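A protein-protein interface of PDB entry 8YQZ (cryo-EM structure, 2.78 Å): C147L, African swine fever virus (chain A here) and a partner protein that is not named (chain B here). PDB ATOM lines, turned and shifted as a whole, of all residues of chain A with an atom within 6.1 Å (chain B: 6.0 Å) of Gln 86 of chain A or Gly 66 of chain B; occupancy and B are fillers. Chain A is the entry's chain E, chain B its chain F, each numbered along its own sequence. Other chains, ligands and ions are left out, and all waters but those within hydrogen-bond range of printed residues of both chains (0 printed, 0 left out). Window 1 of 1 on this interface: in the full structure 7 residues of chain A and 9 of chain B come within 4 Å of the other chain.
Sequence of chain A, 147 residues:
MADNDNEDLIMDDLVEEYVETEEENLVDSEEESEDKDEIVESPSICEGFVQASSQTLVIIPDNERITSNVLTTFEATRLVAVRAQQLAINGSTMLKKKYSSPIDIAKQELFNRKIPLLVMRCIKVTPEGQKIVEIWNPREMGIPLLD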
ATOM      1  N   ALA A  81      31.685  -8.912 -26.948  1.00  0.00           N
ATOM      2  CA  ALA A  81      30.259  -8.937 -27.263  1.00  0.00           C
ATOM      3  C   ALA A  81      29.610 -10.257 -26.862  1.00  0.00           C
ATOM      4  O   ALA A  81      28.522 -10.277 -26.265  1.00  0.00           O
ATOM      5  CB  ALA A  81      30.053  -8.669 -28.749  1.00  0.00           C
ATOM      6  N   VAL A  82      30.264 -11.377 -27.180  1.00  0.00           N
ATOM      7  CA  VAL A  82      29.727 -12.684 -26.816  1.00  0.00           C
ATOM      8  C   VAL A  82      29.630 -12.807 -25.305  1.00  0.00           C
ATOM      9  O   VAL A  82      28.609 -13.248 -24.764  1.00  0.00           O
ATOM     10  CB  VAL A  82      30.589 -13.807 -27.428  1.00  0.00           C
ATOM     11  CG1 VAL A  82      30.231 -15.143 -26.839  1.00  0.00           C
ATOM     12  CG2 VAL A  82      30.416 -13.848 -28.920  1.00  0.00           C
ATOM     13  N   ARG A  83      30.684 -12.397 -24.599  1.00  0.00           N
ATOM     14  CA  ARG A  83      30.676 -12.488 -23.147  1.00  0.00           C
ATOM     15  C   ARG A  83      29.590 -11.613 -22.532  1.00  0.00           C
ATOM     16  O   ARG A  83      28.942 -12.013 -21.564  1.00  0.00           O
ATOM     17  CB  ARG A  83      32.047 -12.107 -22.611  1.00  0.00           C
ATOM     18  CG  ARG A  83      32.220 -12.307 -21.138  1.00  0.00           C
ATOM     19  CD  ARG A  83      31.783 -13.680 -20.716  1.00  0.00           C
ATOM     20  NE  ARG A  83      32.015 -13.887 -19.295  1.00  0.00           N
ATOM     21  CZ  ARG A  83      31.267 -14.646 -18.512  1.00  0.00           C
ATOM     22  NH1 ARG A  83      30.214 -15.290 -18.975  1.00  0.00           N
ATOM     23  NH2 ARG A  83      31.582 -14.756 -17.228  1.00  0.00           N
ATOM     24  N   ALA A  84      29.382 -10.414 -23.068  1.00  0.00           N
ATOM     25  CA  ALA A  84      28.375  -9.523 -22.513  1.00  0.00           C
ATOM     26  C   ALA A  84      26.971 -10.082 -22.695  1.00  0.00           C
ATOM     27  O   ALA A  84      26.144 -10.000 -21.783  1.00  0.00           O
ATOM     28  CB  ALA A  84      28.502  -8.145 -23.150  1.00  0.00           C
ATOM     29  N   GLN A  85      26.677 -10.652 -23.863  1.00  0.00           N
ATOM     30  CA  GLN A  85      25.367 -11.270 -24.047  1.00  0.00           C
ATOM     31  C   GLN A  85      25.180 -12.473 -23.127  1.00  0.00           C
ATOM     32  O   GLN A  85      24.102 -12.668 -22.547  1.00  0.00           O
ATOM     33  CB  GLN A  85      25.178 -11.672 -25.503  1.00  0.00           C
ATOM     34  CG  GLN A  85      23.859 -12.344 -25.794  1.00  0.00           C
ATOM     35  CD  GLN A  85      22.676 -11.429 -25.624  1.00  0.00           C
ATOM     36  OE1 GLN A  85      22.564 -10.410 -26.290  1.00  0.00           O
ATOM     37  NE2 GLN A  85      21.778 -11.795 -24.732  1.00  0.00           N
ATOM     38  N   GLN A  86      26.214 -13.287 -22.964  1.00  0.00           N
ATOM     39  CA  GLN A  86      26.083 -14.430 -22.078  1.00  0.00           C
ATOM     40  C   GLN A  86      25.990 -14.038 -20.610  1.00  0.00           C
ATOM     41  O   GLN A  86      25.469 -14.821 -19.814  1.00  0.00           O
ATOM     42  CB  GLN A  86      27.242 -15.382 -22.310  1.00  0.00           C
ATOM     43  CG  GLN A  86      27.114 -16.131 -23.597  1.00  0.00           C
ATOM     44  CD  GLN A  86      28.356 -16.894 -23.920  1.00  0.00           C
ATOM     45  OE1 GLN A  86      29.379 -16.728 -23.269  1.00  0.00           O
ATOM     46  NE2 GLN A  86      28.280 -17.740 -24.925  1.00  0.00           N
ATOM     47  N   LEU A  87      26.502 -12.867 -20.231  1.00  0.00           N
ATOM     48  CA  LEU A  87      26.242 -12.333 -18.896  1.00  0.00           C
ATOM     49  C   LEU A  87      24.828 -11.796 -18.776  1.00  0.00           C
ATOM     50  O   LEU A  87      24.236 -11.848 -17.698  1.00  0.00           O
ATOM     51  CB  LEU A  87      27.227 -11.229 -18.555  1.00  0.00           C
ATOM     52  CG  LEU A  87      28.603 -11.674 -18.104  1.00  0.00           C
ATOM     53  CD1 LEU A  87      29.594 -10.590 -18.423  1.00  0.00           C
ATOM     54  CD2 LEU A  87      28.585 -11.988 -16.637  1.00  0.00           C
ATOM     55  N   ALA A  88      24.286 -11.242 -19.854  1.00  0.00           N
ATOM     56  CA  ALA A  88      22.872 -10.902 -19.859  1.00  0.00           C
ATOM     57  C   ALA A  88      22.002 -12.140 -19.734  1.00  0.00           C
ATOM     58  O   ALA A  88      20.825 -12.025 -19.383  1.00  0.00           O
ATOM     59  CB  ALA A  88      22.519 -10.130 -21.125  1.00  0.00           C
ATOM     60  N   ILE A  89      22.542 -13.318 -20.033  1.00  0.00           N
ATOM     61  CA  ILE A  89      21.802 -14.561 -19.813  1.00  0.00           C
ATOM     62  C   ILE A  89      22.021 -15.088 -18.399  1.00  0.00           C
ATOM     63  O   ILE A  89      21.068 -15.381 -17.671  1.00  0.00           O
ATOM     64  CB  ILE A  89      22.198 -15.618 -20.859  1.00  0.00           C
ATOM     65  CG1 ILE A  89      21.671 -15.254 -22.244  1.00  0.00           C
ATOM     66  CG2 ILE A  89      21.676 -16.967 -20.460  1.00  0.00           C
ATOM     67  CD1 ILE A  89      22.248 -16.133 -23.349  1.00  0.00           C
ATOM     68  N   ASN A  90      23.280 -15.248 -17.994  1.00  0.00           N
ATOM     69  CA  ASN A  90      23.600 -15.955 -16.757  1.00  0.00           C
ATOM     70  C   ASN A  90      23.840 -15.020 -15.576  1.00  0.00           C
ATOM     71  O   ASN A  90      23.095 -15.046 -14.593  1.00  0.00           O
ATOM     72  CB  ASN A  90      24.828 -16.839 -16.970  1.00  0.00           C
ATOM     73  CG  ASN A  90      24.717 -18.159 -16.264  1.00  0.00           C
ATOM     74  OD1 ASN A  90      23.838 -18.959 -16.563  1.00  0.00           O
ATOM     75  ND2 ASN A  90      25.602 -18.393 -15.306  1.00  0.00           N
ATOM     76  N   GLY A  91      24.876 -14.196 -15.652  1.00  0.00           N
ATOM     77  CA  GLY A  91      25.220 -13.309 -14.563  1.00  0.00           C
ATOM     78  C   GLY A  91      26.353 -13.761 -13.671  1.00  0.00           C
ATOM     79  O   GLY A  91      26.814 -12.971 -12.842  1.00  0.00           O
ATOM     80  N   LEU A 117      36.561 -17.946 -22.711  1.00  0.00           N
ATOM     81  CA  LEU A 117      36.307 -18.248 -24.108  1.00  0.00           C
ATOM     82  C   LEU A 117      37.627 -18.533 -24.805  1.00  0.00           C
ATOM     83  O   LEU A 117      38.698 -18.209 -24.295  1.00  0.00           O
ATOM     84  CB  LEU A 117      35.566 -17.099 -24.798  1.00  0.00           C
ATOM     85  CG  LEU A 117      34.176 -16.732 -24.275  1.00  0.00           C
ATOM     86  CD1 LEU A 117      33.702 -15.430 -24.861  1.00  0.00           C
ATOM     87  CD2 LEU A 117      33.197 -17.826 -24.596  1.00  0.00           C
ATOM     88  N   ILE B  13      22.303 -25.097 -27.430  1.00  0.00           N
ATOM     89  CA  ILE B  13      22.545 -24.862 -26.012  1.00  0.00           C
ATOM     90  C   ILE B  13      22.106 -23.443 -25.694  1.00  0.00           C
ATOM     91  O   ILE B  13      22.644 -22.483 -26.252  1.00  0.00           O
ATOM     92  CB  ILE B  13      24.020 -25.077 -25.646  1.00  0.00           C
ATOM     93  CG1 ILE B  13      24.384 -26.552 -25.722  1.00  0.00           C
ATOM     94  CG2 ILE B  13      24.306 -24.556 -24.277  1.00  0.00           C
ATOM     95  CD1 ILE B  13      25.186 -26.917 -26.887  1.00  0.00           C
ATOM     96  N   PRO B  16      25.331 -21.589 -22.485  1.00  0.00           N
ATOM     97  CA  PRO B  16      26.628 -22.269 -22.635  1.00  0.00           C
ATOM     98  C   PRO B  16      27.502 -22.248 -21.392  1.00  0.00           C
ATOM     99  O   PRO B  16      28.223 -23.220 -21.138  1.00  0.00           O
ATOM    100  CB  PRO B  16      27.269 -21.511 -23.802  1.00  0.00           C
ATOM    101  CG  PRO B  16      26.139 -20.904 -24.526  1.00  0.00           C
ATOM    102  CD  PRO B  16      25.147 -20.537 -23.494  1.00  0.00           C
ATOM    103  N   THR B  17      27.466 -21.172 -20.606  1.00  0.00           N
ATOM    104  CA  THR B  17      28.318 -21.103 -19.424  1.00  0.00           C
ATOM    105  C   THR B  17      27.932 -22.168 -18.407  1.00  0.00           C
ATOM    106  O   THR B  17      28.800 -22.801 -17.798  1.00  0.00           O
ATOM    107  CB  THR B  17      28.234 -19.717 -18.793  1.00  0.00           C
ATOM    108  OG1 THR B  17      28.042 -18.735 -19.815  1.00  0.00           O
ATOM    109  CG2 THR B  17      29.518 -19.400 -18.071  1.00  0.00           C
ATOM    110  N   ILE B  59      29.797 -20.940 -30.500  1.00  0.00           N
ATOM    111  CA  ILE B  59      28.835 -19.865 -30.299  1.00  0.00           C
ATOM    112  C   ILE B  59      28.150 -19.579 -31.621  1.00  0.00           C
ATOM    113  O   ILE B  59      28.799 -19.548 -32.668  1.00  0.00           O
ATOM    114  CB  ILE B  59      29.516 -18.608 -29.735  1.00  0.00           C
ATOM    115  CG1 ILE B  59      30.340 -18.971 -28.508  1.00  0.00           C
ATOM    116  CG2 ILE B  59      28.483 -17.563 -29.367  1.00  0.00           C
ATOM    117  CD1 ILE B  59      29.545 -19.667 -27.447  1.00  0.00           C
ATOM    118  N   MET B  60      26.836 -19.391 -31.577  1.00  0.00           N
ATOM    119  CA  MET B  60      26.074 -19.130 -32.791  1.00  0.00           C
ATOM    120  C   MET B  60      26.542 -17.837 -33.438  1.00  0.00           C
ATOM    121  O   MET B  60      26.899 -16.876 -32.758  1.00  0.00           O
ATOM    122  CB  MET B  60      24.588 -19.059 -32.472  1.00  0.00           C
ATOM    123  CG  MET B  60      23.931 -20.406 -32.344  1.00  0.00           C
ATOM    124  SD  MET B  60      22.158 -20.288 -32.114  1.00  0.00           S
ATOM    125  CE  MET B  60      21.852 -21.705 -31.084  1.00  0.00           C
ATOM    126  N   ASN B  63      23.203 -14.781 -35.517  1.00  0.00           N
ATOM    127  CA  ASN B  63      22.263 -13.983 -34.750  1.00  0.00           C
ATOM    128  C   ASN B  63      22.960 -13.525 -33.482  1.00  0.00           C
ATOM    129  O   ASN B  63      24.036 -14.013 -33.135  1.00  0.00           O
ATOM    130  CB  ASN B  63      20.984 -14.759 -34.431  1.00  0.00           C
ATOM    131  CG  ASN B  63      21.250 -16.062 -33.745  1.00  0.00           C
ATOM    132  OD1 ASN B  63      22.379 -16.397 -33.447  1.00  0.00           O
ATOM    133  ND2 ASN B  63      20.210 -16.818 -33.511  1.00  0.00           N
ATOM    134  N   ASN B  64      22.342 -12.567 -32.796  1.00  0.00           N
ATOM    135  CA  ASN B  64      22.941 -11.941 -31.627  1.00  0.00           C
ATOM    136  C   ASN B  64      22.489 -12.568 -30.322  1.00  0.00           C
ATOM    137  O   ASN B  64      22.551 -11.914 -29.280  1.00  0.00           O
ATOM    138  CB  ASN B  64      22.648 -10.441 -31.621  1.00  0.00           C
ATOM    139  CG  ASN B  64      23.422  -9.679 -32.675  1.00  0.00           C
ATOM    140  OD1 ASN B  64      24.476 -10.109 -33.116  1.00  0.00           O
ATOM    141  ND2 ASN B  64      22.921  -8.523 -33.043  1.00  0.00           N
ATOM    142  N   SER B  65      22.050 -13.821 -30.342  1.00  0.00           N
ATOM    143  CA  SER B  65      21.525 -14.457 -29.142  1.00  0.00           C
ATOM    144  C   SER B  65      22.599 -14.872 -28.149  1.00  0.00           C
ATOM    145  O   SER B  65      22.307 -14.959 -26.957  1.00  0.00           O
ATOM    146  CB  SER B  65      20.685 -15.673 -29.520  1.00  0.00           C
ATOM    147  OG  SER B  65      21.440 -16.609 -30.252  1.00  0.00           O
ATOM    148  N   GLY B  66      23.823 -15.128 -28.595  1.00  0.00           N
ATOM    149  CA  GLY B  66      24.861 -15.571 -27.687  1.00  0.00           C
ATOM    150  C   GLY B  66      24.760 -17.018 -27.283  1.00  0.00           C
ATOM    151  O   GLY B  66      25.367 -17.421 -26.293  1.00  0.00           O
ATOM    152  N   ARG B  67      24.013 -17.815 -28.032  1.00  0.00           N
ATOM    153  CA  ARG B  67      23.722 -19.198 -27.705  1.00  0.00           C
ATOM    154  C   ARG B  67      24.736 -20.118 -28.374  1.00  0.00           C
ATOM    155  O   ARG B  67      25.427 -19.737 -29.317  1.00  0.00           O
ATOM    156  CB  ARG B  67      22.308 -19.552 -28.151  1.00  0.00           C
ATOM    157  CG  ARG B  67      21.245 -19.246 -27.133  1.00  0.00           C
ATOM    158  CD  ARG B  67      19.883 -19.649 -27.641  1.00  0.00           C
ATOM    159  NE  ARG B  67      19.577 -19.053 -28.930  1.00  0.00           N
ATOM    160  CZ  ARG B  67      18.799 -19.609 -29.847  1.00  0.00           C
ATOM    161  NH1 ARG B  67      18.257 -20.800 -29.664  1.00  0.00           N
ATOM    162  NH2 ARG B  67      18.569 -18.957 -30.983  1.00  0.00           N
ATOM    163  N   GLY B  68      24.819 -21.346 -27.870  1.00  0.00           N
ATOM    164  CA  GLY B  68      25.783 -22.313 -28.337  1.00  0.00           C
ATOM    165  C   GLY B  68      25.134 -23.424 -29.144  1.00  0.00           C
ATOM    166  O   GLY B  68      23.918 -23.533 -29.247  1.00  0.00           O
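Printed residues of chain A that touch a printed residue of chain B: Val 82, Gln 85, Gln 86 and Ile 89.
Hydrophobic or aromatic side chains of chain A within 4 Å of the printed part of chain B: Val 82 and Ile 89.
Of the 11 printed residues of chain B, 5 touch a printed residue of chain A.
Printed residues of chain B that touch a printed residue of chain A: Pro 16, Ile 59, Asn 64, Ser 65 and Gly 66.
OG of Ser 65 of chain B sits at hydrogen-bond distance from OD1 of Asn 63 of chain B (3.3 Å).
The guanidinium group (NE) of Arg 67 of chain B sits at hydrogen-bond distance from the side-chain hydroxyl (OG) of Ser 65 of chain B (3.3 Å).
Val 82 of chain A touches Ile 59 of chain B (CG1 to CG2, 3.9 Å).
Gln 85 of chain A touches Ser 65 of chain B.
Gly 66 of chain B touches Gln 85 of chain A.
Pro 16 of chain B touches Gln 86 of chain A (CG to NE2, 3.8 Å).
Ile 59 of chain B touches Gln 86 of chain A.
Ile 89 of chain A touches Ser 65 of chain B (CD1 to O, 3.8 Å).
Of the printed residues of chain B, Gln 86 of chain A touches Pro 16 (3.8 Å), Ile 59 (3.4 Å) and Gly 66 (3.2 Å).
Of chain A, only Gln 85 and Gln 86 come within 4 Å of Gly 66 of chain B.
Printed residues of chain A within 4 Å of Pro 16 of chain B: Gln 86.
Of the printed residues of chain B, Gln 85 of chain A touches Asn 64 (3.3 Å), Ser 65 (3.3 Å) and Gly 66 (3.9 Å).
Of the printed residues of chain A, Ser 65 of chain B touches Gln 85 (3.3 Å) and Ile 89 (3.8 Å).
The nearest residue of chain B that does not touch Gln 86 of chain A is Thr 17 of chain B (4.2 Å).
The side-chain amide oxygen of Gln 85 of chain A sits close to the backbone carbonyl oxygen of Asn 64 of chain B (3.3 Å).
The backbone carbonyl oxygen of Gly 66 of chain B lies within hydrogen-bond range of the side-chain amide nitrogen of Gln 86 of chain A, at 3.2 Å.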
